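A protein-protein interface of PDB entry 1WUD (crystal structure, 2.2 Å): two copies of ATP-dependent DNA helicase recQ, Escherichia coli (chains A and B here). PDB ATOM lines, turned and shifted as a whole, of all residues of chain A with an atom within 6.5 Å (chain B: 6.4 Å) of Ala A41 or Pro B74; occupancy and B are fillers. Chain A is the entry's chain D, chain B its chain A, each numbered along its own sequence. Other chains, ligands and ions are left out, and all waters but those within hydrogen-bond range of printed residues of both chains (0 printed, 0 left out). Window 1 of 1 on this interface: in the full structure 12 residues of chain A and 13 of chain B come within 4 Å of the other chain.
NZ of Lys B73 lies within salt-bridge range of OE2 of Glu A45 (2.7 Å).
The backbone NH (N) of Ala A41 lies within hydrogen-bond range of the side-chain amide oxygen (OD1) of Asn A39. N of Thr A42 lies within hydrogen-bond range of OD1 of Asn A39 (3.0 Å). OG1 of Thr A42 lies within hydrogen-bond range of O of Asn A61, at 2.7 Å. OE1 of Glu A45 lies within hydrogen-bond range of N of Asn A61, 2.8 Å away.
Asn A39 touches Leu B22 (CG to CD1, 3.5 Å). Ala A41 touches Leu B22. Ala A41 touches Pro B74. O of Ala B77 touches CG2 of Ile A44, at 3.8 Å. Leu B78 touches Ile A44. Asn A61 touches Lys B73 (ND2 to CD, 3.5 Å). Asn A61 touches Pro B74 (OD1 to CD, 3.6 Å).
Of the printed residues of chain B, Ala A41 touches Leu B22 (3.98 Å) and Pro B74 (3.2 Å). Of chain A, only Ala A41 (3.2 Å) and Asn A61 (3.6 Å) come within 4 Å of Pro B74. Printed residues of chain B within 4 Å of Ile A44: Ala B77 (3.8 Å) and Leu B78 (3.9 Å). Of the printed residues of chain B, Asn A39 touches Leu B22 (3.5 Å). Of the printed residues of chain A, Leu B78 touches Ile A44 (3.9 Å). Of the printed residues of chain A, Leu B22 touches Asn A39 and Ala A41. Printed residues of chain B within 4 Å of Asn A61: Lys B73 (3.5 Å) and Pro B74 (3.6 Å). Asp A40 touches none of the printed residues of chain B. Met A46 touches none of the printed residues of chain B. The nearest printed residue of chain B that does not touch Ala A41 is Ala B77 (4.3 Å). The nearest residue of chain A that does not touch Pro B74 is Asn A39 (5.3 Å).
Hydrophobic or aromatic side chains of chain B that line the printed part of chain A: Leu B22, Pro B74 and Leu B78. Of the 13 printed residues of chain A, 5 touch a printed residue of chain B. Hydrophobic or aromatic side chains of chain A that line the printed part of chain B: Ala A41 and Ile A44. Among the printed residues, 8 pairs touch across the chains.
No position is printed for both chains.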
ATOM      1  N   PHE A  16     -19.503  -9.296  15.474  1.00  0.00           N
ATOM      2  CA  PHE A  16     -20.085 -10.218  14.510  1.00  0.00           C
ATOM      3  C   PHE A  16     -21.010 -11.229  15.186  1.00  0.00           C
ATOM      4  O   PHE A  16     -22.101 -11.504  14.682  1.00  0.00           O
ATOM      5  CB  PHE A  16     -19.002 -10.929  13.697  1.00  0.00           C
ATOM      6  CG  PHE A  16     -19.546 -11.890  12.672  1.00  0.00           C
ATOM      7  CD1 PHE A  16     -20.285 -11.424  11.579  1.00  0.00           C
ATOM      8  CD2 PHE A  16     -19.337 -13.263  12.807  1.00  0.00           C
ATOM      9  CE1 PHE A  16     -20.793 -12.310  10.627  1.00  0.00           C
ATOM     10  CE2 PHE A  16     -19.839 -14.158  11.861  1.00  0.00           C
ATOM     11  CZ  PHE A  16     -20.571 -13.675  10.764  1.00  0.00           C
ATOM     12  N   ARG A  23     -29.868 -10.861  14.431  1.00  0.00           N
ATOM     13  CA  ARG A  23     -30.530 -11.361  13.229  1.00  0.00           C
ATOM     14  C   ARG A  23     -31.379 -12.597  13.539  1.00  0.00           C
ATOM     15  O   ARG A  23     -32.486 -12.742  13.011  1.00  0.00           O
ATOM     16  CB  ARG A  23     -29.516 -11.683  12.139  1.00  0.00           C
ATOM     17  CG  ARG A  23     -30.161 -12.177  10.841  1.00  0.00           C
ATOM     18  CD  ARG A  23     -29.183 -12.649   9.809  1.00  0.00           C
ATOM     19  NE  ARG A  23     -28.342 -13.736  10.312  1.00  0.00           N
ATOM     20  CZ  ARG A  23     -27.332 -14.267   9.641  1.00  0.00           C
ATOM     21  NH1 ARG A  23     -27.027 -13.819   8.419  1.00  0.00           N
ATOM     22  NH2 ARG A  23     -26.622 -15.245  10.187  1.00  0.00           N
ATOM     23  N   PHE A  38     -30.808 -10.638   6.764  1.00  0.00           N
ATOM     24  CA  PHE A  38     -29.551 -10.316   6.075  1.00  0.00           C
ATOM     25  C   PHE A  38     -28.750 -11.592   5.884  1.00  0.00           C
ATOM     26  O   PHE A  38     -28.808 -12.503   6.719  1.00  0.00           O
ATOM     27  CB  PHE A  38     -28.697  -9.341   6.889  1.00  0.00           C
ATOM     28  CG  PHE A  38     -29.272  -7.971   6.998  1.00  0.00           C
ATOM     29  CD1 PHE A  38     -29.456  -7.184   5.865  1.00  0.00           C
ATOM     30  CD2 PHE A  38     -29.624  -7.453   8.240  1.00  0.00           C
ATOM     31  CE1 PHE A  38     -29.989  -5.910   5.965  1.00  0.00           C
ATOM     32  CE2 PHE A  38     -30.157  -6.172   8.347  1.00  0.00           C
ATOM     33  CZ  PHE A  38     -30.341  -5.404   7.210  1.00  0.00           C
ATOM     34  N   ASN A  39     -27.979 -11.655   4.804  1.00  0.00           N
ATOM     35  CA  ASN A  39     -27.064 -12.773   4.617  1.00  0.00           C
ATOM     36  C   ASN A  39     -25.766 -12.553   5.406  1.00  0.00           C
ATOM     37  O   ASN A  39     -25.536 -11.462   5.947  1.00  0.00           O
ATOM     38  CB  ASN A  39     -26.804 -13.034   3.112  1.00  0.00           C
ATOM     39  CG  ASN A  39     -26.025 -11.916   2.442  1.00  0.00           C
ATOM     40  OD1 ASN A  39     -24.993 -11.475   2.944  1.00  0.00           O
ATOM     41  ND2 ASN A  39     -26.496 -11.483   1.279  1.00  0.00           N
ATOM     42  N   ASP A  40     -24.925 -13.578   5.469  1.00  0.00           N
ATOM     43  CA  ASP A  40     -23.683 -13.503   6.245  1.00  0.00           C
ATOM     44  C   ASP A  40     -22.682 -12.436   5.760  1.00  0.00           C
ATOM     45  O   ASP A  40     -21.999 -11.817   6.571  1.00  0.00           O
ATOM     46  CB  ASP A  40     -23.021 -14.877   6.321  1.00  0.00           C
ATOM     47  CG  ASP A  40     -23.683 -15.789   7.350  1.00  0.00           C
ATOM     48  OD1 ASP A  40     -24.542 -15.302   8.134  1.00  0.00           O
ATOM     49  OD2 ASP A  40     -23.411 -17.001   7.451  1.00  0.00           O
ATOM     50  N   ALA A  41     -22.614 -12.210   4.452  1.00  0.00           N
ATOM     51  CA  ALA A  41     -21.675 -11.221   3.896  1.00  0.00           C
ATOM     52  C   ALA A  41     -22.018  -9.784   4.305  1.00  0.00           C
ATOM     53  O   ALA A  41     -21.123  -8.967   4.527  1.00  0.00           O
ATOM     54  CB  ALA A  41     -21.593 -11.341   2.384  1.00  0.00           C
ATOM     55  N   THR A  42     -23.314  -9.490   4.401  1.00  0.00           N
ATOM     56  CA  THR A  42     -23.793  -8.208   4.923  1.00  0.00           C
ATOM     57  C   THR A  42     -23.363  -8.008   6.387  1.00  0.00           C
ATOM     58  O   THR A  42     -22.913  -6.932   6.776  1.00  0.00           O
ATOM     59  CB  THR A  42     -25.325  -8.156   4.829  1.00  0.00           C
ATOM     60  OG1 THR A  42     -25.723  -8.115   3.453  1.00  0.00           O
ATOM     61  CG2 THR A  42     -25.867  -6.845   5.424  1.00  0.00           C
ATOM     62  N   LEU A  43     -23.508  -9.055   7.186  1.00  0.00           N
ATOM     63  CA  LEU A  43     -23.125  -9.009   8.595  1.00  0.00           C
ATOM     64  C   LEU A  43     -21.612  -8.811   8.754  1.00  0.00           C
ATOM     65  O   LEU A  43     -21.164  -8.027   9.602  1.00  0.00           O
ATOM     66  CB  LEU A  43     -23.579 -10.283   9.316  1.00  0.00           C
ATOM     67  CG  LEU A  43     -25.085 -10.484   9.547  1.00  0.00           C
ATOM     68  CD1 LEU A  43     -25.322 -11.423  10.722  1.00  0.00           C
ATOM     69  CD2 LEU A  43     -25.811  -9.182   9.772  1.00  0.00           C
ATOM     70  N   ILE A  44     -20.839  -9.515   7.922  1.00  0.00           N
ATOM     71  CA  ILE A  44     -19.379  -9.405   7.937  1.00  0.00           C
ATOM     72  C   ILE A  44     -18.932  -7.974   7.635  1.00  0.00           C
ATOM     73  O   ILE A  44     -18.087  -7.425   8.346  1.00  0.00           O
ATOM     74  CB  ILE A  44     -18.732 -10.409   6.953  1.00  0.00           C
ATOM     75  CG1 ILE A  44     -18.854 -11.845   7.488  1.00  0.00           C
ATOM     76  CG2 ILE A  44     -17.265 -10.058   6.714  1.00  0.00           C
ATOM     77  CD1 ILE A  44     -18.838 -12.921   6.400  1.00  0.00           C
ATOM     78  N   GLU A  45     -19.517  -7.373   6.597  1.00  0.00           N
ATOM     79  CA  GLU A  45     -19.233  -5.983   6.262  1.00  0.00           C
ATOM     80  C   GLU A  45     -19.615  -5.039   7.400  1.00  0.00           C
ATOM     81  O   GLU A  45     -18.862  -4.117   7.719  1.00  0.00           O
ATOM     82  CB  GLU A  45     -19.923  -5.565   4.953  1.00  0.00           C
ATOM     83  CG  GLU A  45     -19.894  -4.061   4.700  1.00  0.00           C
ATOM     84  CD  GLU A  45     -19.931  -3.684   3.227  1.00  0.00           C
ATOM     85  OE1 GLU A  45     -20.678  -4.324   2.451  1.00  0.00           O
ATOM     86  OE2 GLU A  45     -19.218  -2.725   2.850  1.00  0.00           O
ATOM     87  N   MET A  46     -20.779  -5.274   8.013  1.00  0.00           N
ATOM     88  CA  MET A  46     -21.187  -4.521   9.199  1.00  0.00           C
ATOM     89  C   MET A  46     -20.144  -4.620  10.307  1.00  0.00           C
ATOM     90  O   MET A  46     -19.775  -3.612  10.906  1.00  0.00           O
ATOM     91  CB  MET A  46     -22.537  -5.006   9.722  1.00  0.00           C
ATOM     92  CG  MET A  46     -23.732  -4.459   8.981  1.00  0.00           C
ATOM     93  SD  MET A  46     -25.383  -5.157   9.748  1.00  0.00           S
ATOM     94  CE  MET A  46     -26.639  -4.470   8.409  1.00  0.00           C
ATOM     95  N   VAL A  60     -23.227  -0.519   2.892  1.00  0.00           N
ATOM     96  CA  VAL A  60     -23.078  -1.955   3.141  1.00  0.00           C
ATOM     97  C   VAL A  60     -23.886  -2.743   2.104  1.00  0.00           C
ATOM     98  O   VAL A  60     -25.067  -2.467   1.891  1.00  0.00           O
ATOM     99  CB  VAL A  60     -23.546  -2.337   4.587  1.00  0.00           C
ATOM    100  CG1 VAL A  60     -23.503  -3.849   4.806  1.00  0.00           C
ATOM    101  CG2 VAL A  60     -22.702  -1.621   5.641  1.00  0.00           C
ATOM    102  N   ASN A  61     -23.246  -3.717   1.457  1.00  0.00           N
ATOM    103  CA  ASN A  61     -23.937  -4.539   0.463  1.00  0.00           C
ATOM    104  C   ASN A  61     -25.052  -5.360   1.088  1.00  0.00           C
ATOM    105  O   ASN A  61     -24.914  -5.870   2.207  1.00  0.00           O
ATOM    106  CB  ASN A  61     -22.958  -5.442  -0.294  1.00  0.00           C
ATOM    107  CG  ASN A  61     -23.199  -5.433  -1.809  1.00  0.00           C
ATOM    108  OD1 ASN A  61     -23.765  -6.376  -2.365  1.00  0.00           O
ATOM    109  ND2 ASN A  61     -22.769  -4.363  -2.474  1.00  0.00           N
ATOM    110  N   LEU B  22     -24.588 -18.388   0.553  1.00  0.00           N
ATOM    111  CA  LEU B  22     -24.607 -16.999   0.104  1.00  0.00           C
ATOM    112  C   LEU B  22     -25.266 -16.886  -1.271  1.00  0.00           C
ATOM    113  O   LEU B  22     -26.129 -16.033  -1.485  1.00  0.00           O
ATOM    114  CB  LEU B  22     -23.194 -16.389   0.085  1.00  0.00           C
ATOM    115  CG  LEU B  22     -23.123 -14.925  -0.394  1.00  0.00           C
ATOM    116  CD1 LEU B  22     -23.917 -13.985   0.523  1.00  0.00           C
ATOM    117  CD2 LEU B  22     -21.679 -14.436  -0.565  1.00  0.00           C
ATOM    118  N   ILE B  26     -28.667 -14.686  -2.358  1.00  0.00           N
ATOM    119  CA  ILE B  26     -28.650 -13.629  -3.369  1.00  0.00           C
ATOM    120  C   ILE B  26     -29.545 -13.988  -4.554  1.00  0.00           C
ATOM    121  O   ILE B  26     -30.248 -13.127  -5.089  1.00  0.00           O
ATOM    122  CB  ILE B  26     -27.189 -13.332  -3.826  1.00  0.00           C
ATOM    123  CG1 ILE B  26     -26.425 -12.594  -2.716  1.00  0.00           C
ATOM    124  CG2 ILE B  26     -27.169 -12.509  -5.120  1.00  0.00           C
ATOM    125  CD1 ILE B  26     -24.925 -12.637  -2.865  1.00  0.00           C
ATOM    126  N   LEU B  68     -18.762  -9.473 -11.370  1.00  0.00           N
ATOM    127  CA  LEU B  68     -17.953  -8.867 -10.318  1.00  0.00           C
ATOM    128  C   LEU B  68     -18.640  -7.607  -9.756  1.00  0.00           C
ATOM    129  O   LEU B  68     -18.763  -7.445  -8.538  1.00  0.00           O
ATOM    130  CB  LEU B  68     -16.540  -8.545 -10.837  1.00  0.00           C
ATOM    131  CG  LEU B  68     -15.569  -7.827  -9.883  1.00  0.00           C
ATOM    132  CD1 LEU B  68     -15.134  -8.736  -8.733  1.00  0.00           C
ATOM    133  CD2 LEU B  68     -14.361  -7.305 -10.643  1.00  0.00           C
ATOM    134  N   ARG B  70     -21.881  -6.885  -9.995  1.00  0.00           N
ATOM    135  CA  ARG B  70     -23.183  -7.240  -9.433  1.00  0.00           C
ATOM    136  C   ARG B  70     -23.093  -8.047  -8.129  1.00  0.00           C
ATOM    137  O   ARG B  70     -23.835  -7.780  -7.177  1.00  0.00           O
ATOM    138  CB  ARG B  70     -24.000  -8.014 -10.469  1.00  0.00           C
ATOM    139  CG  ARG B  70     -25.489  -8.043 -10.206  1.00  0.00           C
ATOM    140  CD  ARG B  70     -26.243  -6.817 -10.704  1.00  0.00           C
ATOM    141  NE  ARG B  70     -27.630  -6.812 -10.242  1.00  0.00           N
ATOM    142  CZ  ARG B  70     -28.137  -5.928  -9.385  1.00  0.00           C
ATOM    143  NH1 ARG B  70     -27.376  -4.957  -8.883  1.00  0.00           N
ATOM    144  NH2 ARG B  70     -29.412  -6.011  -9.030  1.00  0.00           N
ATOM    145  N   PHE B  71     -22.188  -9.030  -8.097  1.00  0.00           N
ATOM    146  CA  PHE B  71     -22.147 -10.017  -7.012  1.00  0.00           C
ATOM    147  C   PHE B  71     -20.807 -10.115  -6.293  1.00  0.00           C
ATOM    148  O   PHE B  71     -20.688 -10.853  -5.323  1.00  0.00           O
ATOM    149  CB  PHE B  71     -22.515 -11.407  -7.538  1.00  0.00           C
ATOM    150  CG  PHE B  71     -23.788 -11.446  -8.309  1.00  0.00           C
ATOM    151  CD1 PHE B  71     -24.989 -11.074  -7.714  1.00  0.00           C
ATOM    152  CD2 PHE B  71     -23.798 -11.871  -9.634  1.00  0.00           C
ATOM    153  CE1 PHE B  71     -26.178 -11.115  -8.430  1.00  0.00           C
ATOM    154  CE2 PHE B  71     -24.985 -11.911 -10.362  1.00  0.00           C
ATOM    155  CZ  PHE B  71     -26.175 -11.538  -9.759  1.00  0.00           C
ATOM    156  N   GLY B  72     -19.809  -9.369  -6.762  1.00  0.00           N
ATOM    157  CA  GLY B  72     -18.439  -9.550  -6.314  1.00  0.00           C
ATOM    158  C   GLY B  72     -18.197  -9.244  -4.852  1.00  0.00           C
ATOM    159  O   GLY B  72     -17.596 -10.050  -4.131  1.00  0.00           O
ATOM    160  N   LYS B  73     -18.657  -8.074  -4.417  1.00  0.00           N
ATOM    161  CA  LYS B  73     -18.413  -7.586  -3.060  1.00  0.00           C
ATOM    162  C   LYS B  73     -18.760  -8.612  -1.971  1.00  0.00           C
ATOM    163  O   LYS B  73     -17.892  -8.971  -1.174  1.00  0.00           O
ATOM    164  CB  LYS B  73     -19.139  -6.254  -2.822  1.00  0.00           C
ATOM    165  CG  LYS B  73     -18.611  -5.454  -1.641  1.00  0.00           C
ATOM    166  CD  LYS B  73     -19.469  -4.225  -1.385  1.00  0.00           C
ATOM    167  CE  LYS B  73     -18.871  -3.360  -0.289  1.00  0.00           C
ATOM    168  NZ  LYS B  73     -19.839  -2.321   0.202  1.00  0.00           N
ATOM    169  N   PRO B  74     -20.012  -9.090  -1.930  1.00  0.00           N
ATOM    170  CA  PRO B  74     -20.420 -10.032  -0.872  1.00  0.00           C
ATOM    171  C   PRO B  74     -19.604 -11.332  -0.873  1.00  0.00           C
ATOM    172  O   PRO B  74     -19.248 -11.819   0.201  1.00  0.00           O
ATOM    173  CB  PRO B  74     -21.907 -10.300  -1.167  1.00  0.00           C
ATOM    174  CG  PRO B  74     -22.163  -9.776  -2.549  1.00  0.00           C
ATOM    175  CD  PRO B  74     -21.127  -8.745  -2.835  1.00  0.00           C
ATOM    176  N   PHE B  75     -19.282 -11.862  -2.052  1.00  0.00           N
ATOM    177  CA  PHE B  75     -18.493 -13.094  -2.124  1.00  0.00           C
ATOM    178  C   PHE B  75     -17.062 -12.879  -1.634  1.00  0.00           C
ATOM    179  O   PHE B  75     -16.553 -13.670  -0.839  1.00  0.00           O
ATOM    180  CB  PHE B  75     -18.532 -13.702  -3.528  1.00  0.00           C
ATOM    181  CG  PHE B  75     -19.805 -14.453  -3.818  1.00  0.00           C
ATOM    182  CD1 PHE B  75     -19.907 -15.813  -3.540  1.00  0.00           C
ATOM    183  CD2 PHE B  75     -20.914 -13.791  -4.332  1.00  0.00           C
ATOM    184  CE1 PHE B  75     -21.103 -16.507  -3.784  1.00  0.00           C
ATOM    185  CE2 PHE B  75     -22.100 -14.468  -4.584  1.00  0.00           C
ATOM    186  CZ  PHE B  75     -22.196 -15.827  -4.313  1.00  0.00           C
ATOM    187  N   MET B  76     -16.438 -11.791  -2.085  1.00  0.00           N
ATOM    188  CA  MET B  76     -15.117 -11.391  -1.590  1.00  0.00           C
ATOM    189  C   MET B  76     -15.082 -11.176  -0.083  1.00  0.00           C
ATOM    190  O   MET B  76     -14.154 -11.628   0.577  1.00  0.00           O
ATOM    191  CB  MET B  76     -14.622 -10.142  -2.303  1.00  0.00           C
ATOM    192  CG  MET B  76     -14.235 -10.389  -3.739  1.00  0.00           C
ATOM    193  SD  MET B  76     -13.348  -8.843  -4.525  1.00  0.00           S
ATOM    194  CE  MET B  76     -14.899  -7.772  -4.924  1.00  0.00           C
ATOM    195  N   ALA B  77     -16.094 -10.488   0.456  1.00  0.00           N
ATOM    196  CA  ALA B  77     -16.218 -10.299   1.910  1.00  0.00           C
ATOM    197  C   ALA B  77     -16.277 -11.632   2.652  1.00  0.00           C
ATOM    198  O   ALA B  77     -15.648 -11.798   3.698  1.00  0.00           O
ATOM    199  CB  ALA B  77     -17.454  -9.453   2.247  1.00  0.00           C
ATOM    200  N   LEU B  78     -17.036 -12.579   2.102  1.00  0.00           N
ATOM    201  CA  LEU B  78     -17.180 -13.903   2.706  1.00  0.00           C
ATOM    202  C   LEU B  78     -15.861 -14.685   2.671  1.00  0.00           C
ATOM    203  O   LEU B  78     -15.452 -15.279   3.670  1.00  0.00           O
ATOM    204  CB  LEU B  78     -18.297 -14.692   2.007  1.00  0.00           C
ATOM    205  CG  LEU B  78     -18.653 -16.086   2.555  1.00  0.00           C
ATOM    206  CD1 LEU B  78     -19.106 -16.016   4.009  1.00  0.00           C
ATOM    207  CD2 LEU B  78     -19.723 -16.759   1.690  1.00  0.00           C
ATOM    208  N   ILE B  79     -15.192 -14.668   1.525  1.00  0.00           N
ATOM    209  CA  ILE B  79     -13.927 -15.369   1.386  1.00  0.00           C
ATOM    210  C   ILE B  79     -12.847 -14.755   2.299  1.00  0.00           C
ATOM    211  O   ILE B  79     -12.147 -15.478   3.005  1.00  0.00           O
ATOM    212  CB  ILE B  79     -13.474 -15.396  -0.089  1.00  0.00           C
ATOM    213  CG1 ILE B  79     -14.461 -16.218  -0.935  1.00  0.00           C
ATOM    214  CG2 ILE B  79     -12.061 -15.969  -0.201  1.00  0.00           C
ATOM    215  CD1 ILE B  79     -14.377 -15.962  -2.452  1.00  0.00           C
